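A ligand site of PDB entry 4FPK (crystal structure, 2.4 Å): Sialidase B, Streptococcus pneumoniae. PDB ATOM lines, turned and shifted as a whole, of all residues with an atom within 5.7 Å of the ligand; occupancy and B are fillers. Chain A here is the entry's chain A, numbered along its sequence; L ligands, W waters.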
ATOM      1  N   ARG A 245      -4.020  18.514   4.604  1.00  0.00           N
ATOM      2  CA  ARG A 245      -4.112  19.723   3.810  1.00  0.00           C
ATOM      3  C   ARG A 245      -2.787  20.465   3.793  1.00  0.00           C
ATOM      4  O   ARG A 245      -1.893  20.196   4.593  1.00  0.00           O
ATOM      5  CB  ARG A 245      -5.231  20.652   4.343  1.00  0.00           C
ATOM      6  CG  ARG A 245      -6.637  20.332   3.808  1.00  0.00           C
ATOM      7  CD  ARG A 245      -7.501  21.610   3.691  1.00  0.00           C
ATOM      8  NE  ARG A 245      -6.892  22.631   2.828  1.00  0.00           N
ATOM      9  CZ  ARG A 245      -7.373  23.854   2.652  1.00  0.00           C
ATOM     10  NH1 ARG A 245      -8.492  24.229   3.271  1.00  0.00           N
ATOM     11  NH2 ARG A 245      -6.744  24.708   1.848  1.00  0.00           N
ATOM     12  N   ILE A 246      -2.664  21.408   2.864  1.00  0.00           N
ATOM     13  CA  ILE A 246      -1.517  22.306   2.804  1.00  0.00           C
ATOM     14  C   ILE A 246      -0.195  21.560   2.565  1.00  0.00           C
ATOM     15  O   ILE A 246       0.697  21.570   3.423  1.00  0.00           O
ATOM     16  CB  ILE A 246      -1.406  23.197   4.089  1.00  0.00           C
ATOM     17  CG1 ILE A 246      -2.776  23.609   4.650  1.00  0.00           C
ATOM     18  CG2 ILE A 246      -0.590  24.410   3.801  1.00  0.00           C
ATOM     19  CD1 ILE A 246      -3.655  24.482   3.736  1.00  0.00           C
ATOM     20  N   ASP A 270      -9.701  24.332   9.101  1.00  0.00           N
ATOM     21  CA  ASP A 270      -8.612  25.172   9.651  1.00  0.00           C
ATOM     22  C   ASP A 270      -8.778  25.226  11.176  1.00  0.00           C
ATOM     23  O   ASP A 270      -9.880  25.080  11.682  1.00  0.00           O
ATOM     24  CB  ASP A 270      -8.724  26.606   9.113  1.00  0.00           C
ATOM     25  CG  ASP A 270      -8.209  26.770   7.669  1.00  0.00           C
ATOM     26  OD1 ASP A 270      -8.148  27.921   7.187  1.00  0.00           O
ATOM     27  OD2 ASP A 270      -7.879  25.775   7.003  1.00  0.00           O
ATOM     28  N   SER A 271      -7.694  25.453  11.909  1.00  0.00           N
ATOM     29  CA  SER A 271      -7.833  25.717  13.344  1.00  0.00           C
ATOM     30  C   SER A 271      -8.956  26.751  13.614  1.00  0.00           C
ATOM     31  O   SER A 271      -9.032  27.760  12.927  1.00  0.00           O
ATOM     32  CB  SER A 271      -6.514  26.217  13.935  1.00  0.00           C
ATOM     33  OG  SER A 271      -5.533  25.189  13.902  1.00  0.00           O
ATOM     34  N   LYS A 272      -9.829  26.518  14.596  1.00  0.00           N
ATOM     35  CA  LYS A 272      -9.670  25.504  15.640  1.00  0.00           C
ATOM     36  C   LYS A 272      -9.968  24.049  15.271  1.00  0.00           C
ATOM     37  O   LYS A 272     -10.967  23.720  14.618  1.00  0.00           O
ATOM     38  CB  LYS A 272     -10.490  25.908  16.871  1.00  0.00           C
ATOM     39  CG  LYS A 272     -11.971  26.011  16.595  1.00  0.00           C
ATOM     40  CD  LYS A 272     -12.743  26.598  17.776  1.00  0.00           C
ATOM     41  CE  LYS A 272     -14.260  26.606  17.475  1.00  0.00           C
ATOM     42  NZ  LYS A 272     -15.112  26.667  18.706  1.00  0.00           N
ATOM     43  N   ILE A 326      -0.542  24.987  11.886  1.00  0.00           N
ATOM     44  CA  ILE A 326      -1.176  25.093  10.574  1.00  0.00           C
ATOM     45  C   ILE A 326      -0.238  25.835   9.641  1.00  0.00           C
ATOM     46  O   ILE A 326       0.439  26.766  10.063  1.00  0.00           O
ATOM     47  CB  ILE A 326      -2.596  25.777  10.653  1.00  0.00           C
ATOM     48  CG1 ILE A 326      -3.224  25.941   9.275  1.00  0.00           C
ATOM     49  CG2 ILE A 326      -2.529  27.113  11.375  1.00  0.00           C
ATOM     50  CD1 ILE A 326      -4.647  26.463   9.343  1.00  0.00           C
ATOM     51  N   ASP A 327      -0.168  25.395   8.387  1.00  0.00           N
ATOM     52  CA  ASP A 327       0.671  26.060   7.372  1.00  0.00           C
ATOM     53  C   ASP A 327       2.185  25.940   7.606  1.00  0.00           C
ATOM     54  O   ASP A 327       2.811  26.800   8.226  1.00  0.00           O
ATOM     55  CB  ASP A 327       0.260  27.534   7.199  1.00  0.00           C
ATOM     56  CG  ASP A 327      -1.115  27.675   6.641  1.00  0.00           C
ATOM     57  OD1 ASP A 327      -1.696  26.626   6.258  1.00  0.00           O
ATOM     58  OD2 ASP A 327      -1.621  28.804   6.571  1.00  0.00           O
ATOM     59  N   ASP A 344       2.627  28.076  11.481  1.00  0.00           N
ATOM     60  CA  ASP A 344       1.833  28.850  12.423  1.00  0.00           C
ATOM     61  C   ASP A 344       1.531  27.980  13.644  1.00  0.00           C
ATOM     62  O   ASP A 344       1.405  26.762  13.513  1.00  0.00           O
ATOM     63  CB  ASP A 344       0.529  29.349  11.794  1.00  0.00           C
ATOM     64  CG  ASP A 344       0.752  30.277  10.609  1.00  0.00           C
ATOM     65  OD1 ASP A 344       1.674  31.120  10.645  1.00  0.00           O
ATOM     66  OD2 ASP A 344      -0.005  30.177   9.630  1.00  0.00           O
ATOM     67  N   MET A 346      -1.107  27.773  17.186  1.00  0.00           N
ATOM     68  CA  MET A 346      -2.298  28.296  17.847  1.00  0.00           C
ATOM     69  C   MET A 346      -2.520  27.585  19.165  1.00  0.00           C
ATOM     70  O   MET A 346      -2.494  26.361  19.229  1.00  0.00           O
ATOM     71  CB  MET A 346      -3.529  28.117  16.952  1.00  0.00           C
ATOM     72  CG  MET A 346      -3.255  28.335  15.461  1.00  0.00           C
ATOM     73  SD  MET A 346      -4.496  29.297  14.607  1.00  0.00           S
ATOM     74  CE  MET A 346      -4.391  30.825  15.530  1.00  0.00           C
ATOM     75  N   GLY A 351      -8.214  29.962  16.752  1.00  0.00           N
ATOM     76  CA  GLY A 351      -7.943  29.934  15.325  1.00  0.00           C
ATOM     77  C   GLY A 351      -7.867  31.339  14.718  1.00  0.00           C
ATOM     78  O   GLY A 351      -7.409  32.265  15.369  1.00  0.00           O
ATOM     79  N   ASN A 352      -8.321  31.463  13.470  1.00  0.00           N
ATOM     80  CA  ASN A 352      -8.319  32.742  12.747  1.00  0.00           C
ATOM     81  C   ASN A 352      -9.392  33.689  13.280  1.00  0.00           C
ATOM     82  O   ASN A 352      -9.140  34.874  13.484  1.00  0.00           O
ATOM     83  CB  ASN A 352      -8.527  32.492  11.246  1.00  0.00           C
ATOM     84  CG  ASN A 352      -8.169  33.700  10.374  1.00  0.00           C
ATOM     85  OD1 ASN A 352      -8.406  34.848  10.756  1.00  0.00           O
ATOM     86  ND2 ASN A 352      -7.609  33.441   9.193  1.00  0.00           N
ATOM     87  N   ASN A 353     -10.593  33.145  13.504  1.00  0.00           N
ATOM     88  CA  ASN A 353     -11.744  33.907  14.018  1.00  0.00           C
ATOM     89  C   ASN A 353     -11.427  34.612  15.333  1.00  0.00           C
ATOM     90  O   ASN A 353     -11.473  35.842  15.421  1.00  0.00           O
ATOM     91  CB  ASN A 353     -12.947  32.990  14.250  1.00  0.00           C
ATOM     92  CG  ASN A 353     -13.132  31.973  13.141  1.00  0.00           C
ATOM     93  OD1 ASN A 353     -12.967  32.281  11.961  1.00  0.00           O
ATOM     94  ND2 ASN A 353     -13.482  30.744  13.520  1.00  0.00           N
ATOM     95  N   TYR A 489       1.149  35.884   9.187  1.00  0.00           N
ATOM     96  CA  TYR A 489       0.711  34.549   8.800  1.00  0.00           C
ATOM     97  C   TYR A 489       1.651  33.947   7.793  1.00  0.00           C
ATOM     98  O   TYR A 489       1.903  34.536   6.747  1.00  0.00           O
ATOM     99  CB  TYR A 489      -0.708  34.602   8.208  1.00  0.00           C
ATOM    100  CG  TYR A 489      -1.773  34.800   9.246  1.00  0.00           C
ATOM    101  CD1 TYR A 489      -2.228  33.736  10.010  1.00  0.00           C
ATOM    102  CD2 TYR A 489      -2.326  36.063   9.476  1.00  0.00           C
ATOM    103  CE1 TYR A 489      -3.208  33.908  10.972  1.00  0.00           C
ATOM    104  CE2 TYR A 489      -3.302  36.244  10.439  1.00  0.00           C
ATOM    105  CZ  TYR A 489      -3.745  35.163  11.181  1.00  0.00           C
ATOM    106  OH  TYR A 489      -4.713  35.339  12.133  1.00  0.00           O
ATOM    107  N   TYR A 509       2.299  36.942   5.487  1.00  0.00           N
ATOM    108  CA  TYR A 509       1.369  38.021   5.169  1.00  0.00           C
ATOM    109  C   TYR A 509       0.625  38.532   6.394  1.00  0.00           C
ATOM    110  O   TYR A 509       0.479  37.834   7.389  1.00  0.00           O
ATOM    111  CB  TYR A 509       0.384  37.595   4.089  1.00  0.00           C
ATOM    112  CG  TYR A 509      -0.559  36.467   4.488  1.00  0.00           C
ATOM    113  CD1 TYR A 509      -1.845  36.738   4.967  1.00  0.00           C
ATOM    114  CD2 TYR A 509      -0.163  35.143   4.360  1.00  0.00           C
ATOM    115  CE1 TYR A 509      -2.716  35.697   5.318  1.00  0.00           C
ATOM    116  CE2 TYR A 509      -1.021  34.106   4.700  1.00  0.00           C
ATOM    117  CZ  TYR A 509      -2.293  34.380   5.179  1.00  0.00           C
ATOM    118  OH  TYR A 509      -3.129  33.342   5.519  1.00  0.00           O
ATOM    119  N   THR A 539      -5.960  37.056   2.272  1.00  0.00           N
ATOM    120  CA  THR A 539      -5.158  35.869   2.538  1.00  0.00           C
ATOM    121  C   THR A 539      -4.112  35.802   1.439  1.00  0.00           C
ATOM    122  O   THR A 539      -4.330  35.166   0.406  1.00  0.00           O
ATOM    123  CB  THR A 539      -6.007  34.583   2.512  1.00  0.00           C
ATOM    124  OG1 THR A 539      -7.105  34.723   3.416  1.00  0.00           O
ATOM    125  CG2 THR A 539      -5.168  33.378   2.935  1.00  0.00           C
ATOM    126  N   GLU A 541      -1.206  34.463   0.418  1.00  0.00           N
ATOM    127  CA  GLU A 541      -0.199  33.419   0.404  1.00  0.00           C
ATOM    128  C   GLU A 541       0.706  33.618  -0.803  1.00  0.00           C
ATOM    129  O   GLU A 541       0.259  33.663  -1.946  1.00  0.00           O
ATOM    130  CB  GLU A 541      -0.849  32.035   0.394  1.00  0.00           C
ATOM    131  CG  GLU A 541      -1.518  31.689   1.712  1.00  0.00           C
ATOM    132  CD  GLU A 541      -2.757  30.844   1.529  1.00  0.00           C
ATOM    133  OE1 GLU A 541      -3.247  30.273   2.525  1.00  0.00           O
ATOM    134  OE2 GLU A 541      -3.237  30.758   0.379  1.00  0.00           O
ATOM    135  N   ARG A 557      -1.487  35.206  -3.876  1.00  0.00           N
ATOM    136  CA  ARG A 557      -2.942  35.166  -3.911  1.00  0.00           C
ATOM    137  C   ARG A 557      -3.568  36.503  -3.512  1.00  0.00           C
ATOM    138  O   ARG A 557      -3.088  37.160  -2.598  1.00  0.00           O
ATOM    139  CB  ARG A 557      -3.394  34.082  -2.948  1.00  0.00           C
ATOM    140  CG  ARG A 557      -4.858  34.056  -2.600  1.00  0.00           C
ATOM    141  CD  ARG A 557      -5.121  32.913  -1.608  1.00  0.00           C
ATOM    142  NE  ARG A 557      -6.489  32.930  -1.111  1.00  0.00           N
ATOM    143  CZ  ARG A 557      -6.965  32.050  -0.235  1.00  0.00           C
ATOM    144  NH1 ARG A 557      -6.190  31.082   0.236  1.00  0.00           N
ATOM    145  NH2 ARG A 557      -8.230  32.136   0.152  1.00  0.00           N
ATOM    146  N   GLY A 590      -9.652  33.448  -3.962  1.00  0.00           N
ATOM    147  CA  GLY A 590      -8.321  33.031  -4.391  1.00  0.00           C
ATOM    148  C   GLY A 590      -7.834  31.740  -3.759  1.00  0.00           C
ATOM    149  O   GLY A 590      -8.477  31.217  -2.843  1.00  0.00           O
ATOM    150  N   ARG A 619     -12.293  26.038  -7.034  1.00  0.00           N
ATOM    151  CA  ARG A 619     -10.963  25.463  -6.982  1.00  0.00           C
ATOM    152  C   ARG A 619     -10.903  24.194  -7.816  1.00  0.00           C
ATOM    153  O   ARG A 619     -11.041  23.088  -7.307  1.00  0.00           O
ATOM    154  CB  ARG A 619     -10.545  25.212  -5.530  1.00  0.00           C
ATOM    155  CG  ARG A 619     -10.166  26.524  -4.822  1.00  0.00           C
ATOM    156  CD  ARG A 619      -9.846  26.344  -3.362  1.00  0.00           C
ATOM    157  NE  ARG A 619      -9.348  27.576  -2.764  1.00  0.00           N
ATOM    158  CZ  ARG A 619      -9.011  27.697  -1.466  1.00  0.00           C
ATOM    159  NH1 ARG A 619      -9.139  26.644  -0.654  1.00  0.00           N
ATOM    160  NH2 ARG A 619      -8.570  28.851  -0.991  1.00  0.00           N
ATOM    161  N   TYR A 653      -4.815  23.784  -3.099  1.00  0.00           N
ATOM    162  CA  TYR A 653      -3.441  24.128  -2.702  1.00  0.00           C
ATOM    163  C   TYR A 653      -2.465  23.150  -3.342  1.00  0.00           C
ATOM    164  O   TYR A 653      -2.821  21.996  -3.621  1.00  0.00           O
ATOM    165  CB  TYR A 653      -3.263  24.091  -1.177  1.00  0.00           C
ATOM    166  CG  TYR A 653      -3.724  25.350  -0.459  1.00  0.00           C
ATOM    167  CD1 TYR A 653      -4.957  25.922  -0.745  1.00  0.00           C
ATOM    168  CD2 TYR A 653      -2.928  25.942   0.519  1.00  0.00           C
ATOM    169  CE1 TYR A 653      -5.389  27.061  -0.086  1.00  0.00           C
ATOM    170  CE2 TYR A 653      -3.368  27.085   1.179  1.00  0.00           C
ATOM    171  CZ  TYR A 653      -4.596  27.632   0.871  1.00  0.00           C
ATOM    172  OH  TYR A 653      -5.056  28.764   1.521  1.00  0.00           O
ATOM    173  N   SER A 673     -11.141  22.590  -1.829  1.00  0.00           N
ATOM    174  CA  SER A 673     -10.958  22.728  -0.394  1.00  0.00           C
ATOM    175  C   SER A 673     -11.624  24.002   0.123  1.00  0.00           C
ATOM    176  O   SER A 673     -11.507  24.355   1.293  1.00  0.00           O
ATOM    177  CB  SER A 673      -9.475  22.692  -0.014  1.00  0.00           C
ATOM    178  OG  SER A 673      -8.752  23.783  -0.557  1.00  0.00           O
ATOM    179  N   TRP A 674     -12.308  24.710  -0.779  1.00  0.00           N
ATOM    180  CA  TRP A 674     -13.106  25.858  -0.385  1.00  0.00           C
ATOM    181  C   TRP A 674     -14.570  25.430  -0.223  1.00  0.00           C
ATOM    182  O   TRP A 674     -15.231  25.842   0.721  1.00  0.00           O
ATOM    183  CB  TRP A 674     -12.992  27.009  -1.391  1.00  0.00           C
ATOM    184  CG  TRP A 674     -13.708  28.245  -0.925  1.00  0.00           C
ATOM    185  CD1 TRP A 674     -15.007  28.587  -1.173  1.00  0.00           C
ATOM    186  CD2 TRP A 674     -13.170  29.304  -0.118  1.00  0.00           C
ATOM    187  NE1 TRP A 674     -15.316  29.782  -0.575  1.00  0.00           N
ATOM    188  CE2 TRP A 674     -14.199  30.249   0.081  1.00  0.00           C
ATOM    189  CE3 TRP A 674     -11.917  29.540   0.468  1.00  0.00           C
ATOM    190  CZ2 TRP A 674     -14.023  31.413   0.839  1.00  0.00           C
ATOM    191  CZ3 TRP A 674     -11.732  30.699   1.215  1.00  0.00           C
ATOM    192  CH2 TRP A 674     -12.792  31.616   1.394  1.00  0.00           C
HETATM  193  C1  LIG L   1      -6.909  29.422  11.342  1.00  0.00           C
HETATM  194  C2  LIG L   1      -5.933  29.878  10.258  1.00  0.00           C
HETATM  195  C3  LIG L   1      -6.351  30.028   8.971  1.00  0.00           C
HETATM  196  C4  LIG L   1      -4.553  30.138  10.621  1.00  0.00           C
HETATM  197  C5  LIG L   1      -3.649  30.540   9.637  1.00  0.00           C
HETATM  198  C6  LIG L   1      -4.087  30.705   8.281  1.00  0.00           C
HETATM  199  C7  LIG L   1      -5.397  30.459   7.947  1.00  0.00           C
HETATM  200  C8  LIG L   1      -5.875  30.605   6.531  1.00  0.00           C
HETATM  201  N1  LIG L   1      -6.640  29.519   6.033  1.00  0.00           N
HETATM  202  C9  LIG L   1      -6.678  29.529   4.551  1.00  0.00           C
HETATM  203  C10 LIG L   1      -7.129  28.247   3.888  1.00  0.00           C
HETATM  204  S1  LIG L   1      -8.518  28.361   2.757  1.00  0.00           S
HETATM  205  O1  LIG L   1      -8.709  27.028   2.070  1.00  0.00           O
HETATM  206  O2  LIG L   1      -8.277  29.436   1.711  1.00  0.00           O
HETATM  207  O3  LIG L   1      -9.694  28.693   3.566  1.00  0.00           O
HETATM  208  O   HOH W   1      -4.500  27.400   5.435  1.00  0.00           O
HETATM  209  O   HOH W   2      -9.792  31.985   4.446  1.00  0.00           O
HETATM  210  O   HOH W   3     -10.687  26.605   5.080  1.00  0.00           O
HETATM  211  O   HOH W   4      -0.729  30.938   7.330  1.00  0.00           O
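NH2 of Arg 245 lies within salt-bridge range of O1 of the ligand (3.0 Å). An oxygen (O2) of the ligand lies within salt-bridge range of the guanidinium group of Arg 557 (3.0 Å). The guanidinium group of Arg 619 lies within salt-bridge range of an oxygen (O2) of the ligand (2.8 Å). OH of Tyr 653 lies close to O2 of the ligand (3.3 Å). The side-chain carboxylate (OD1) of Asp 270 is in salt-bridge range of a nitrogen (N1) of the ligand (2.5 Å).
The guanidinium group (NH1) of Arg 557 lies within hydrogen-bond range of the side-chain hydroxyl (OH) of Tyr 653, 2.9 Å away. N of Tyr 489 is in hydrogen-bond range of O of Tyr 509, at 2.7 Å. The side-chain carboxylate (OE2) of Glu 541 lies within salt-bridge range of the guanidinium group (NH1) of Arg 557, 3.0 Å away. The guanidinium group of Arg 245 is in hydrogen-bond range of the side-chain hydroxyl of Ser 673 (3.3 Å). NH2 of Arg 619 is in hydrogen-bond range of O of Gly 590 (3.0 Å). OH of Tyr 653 is in hydrogen-bond range of OE1 of Glu 541. NH2 of Arg 557 lies close to O of Gly 590 (3.1 Å). The guanidinium group (NH1) of Arg 619 is in hydrogen-bond range of the side-chain hydroxyl (OG) of Ser 673 (2.9 Å).
O of Ser 271 touches C1 of the ligand (3.1 Å). Ile 326 touches the ligand (CG2 to C4, 3.7 Å). OD2 of Asp 327 touches C6 of the ligand (3.6 Å). OD2 of Asp 344 touches C5 of the ligand, at 3.7 Å. Gly 351 touches the ligand (C to C1, 3.999 Å). N of Asn 352 touches C1 of the ligand, at 3.3 Å. Tyr 489 touches the ligand. Tyr 509 touches the ligand. O of Ser 673 touches O1 of the ligand (3.9 Å). CZ3 of Trp 674 touches O3 of the ligand, 3.7 Å away. 15 residues have an atom within 4 Å of the ligand: Arg 245, Asp 270, Ser 271, Ile 326, Asp 327, Asp 344, Gly 351, Asn 352, Tyr 489, Tyr 509, Arg 557, Arg 619, Tyr 653, Ser 673 and Trp 674.
Water W1 lies within hydrogen-bond range of OD1 of Asp 327 (3.0 Å) and N1 of the ligand (3.1 Å). Water W4 lies within hydrogen-bond range of OD2 of Asp 327 (2.4 Å) and OD2 of Asp 344 (2.5 Å).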
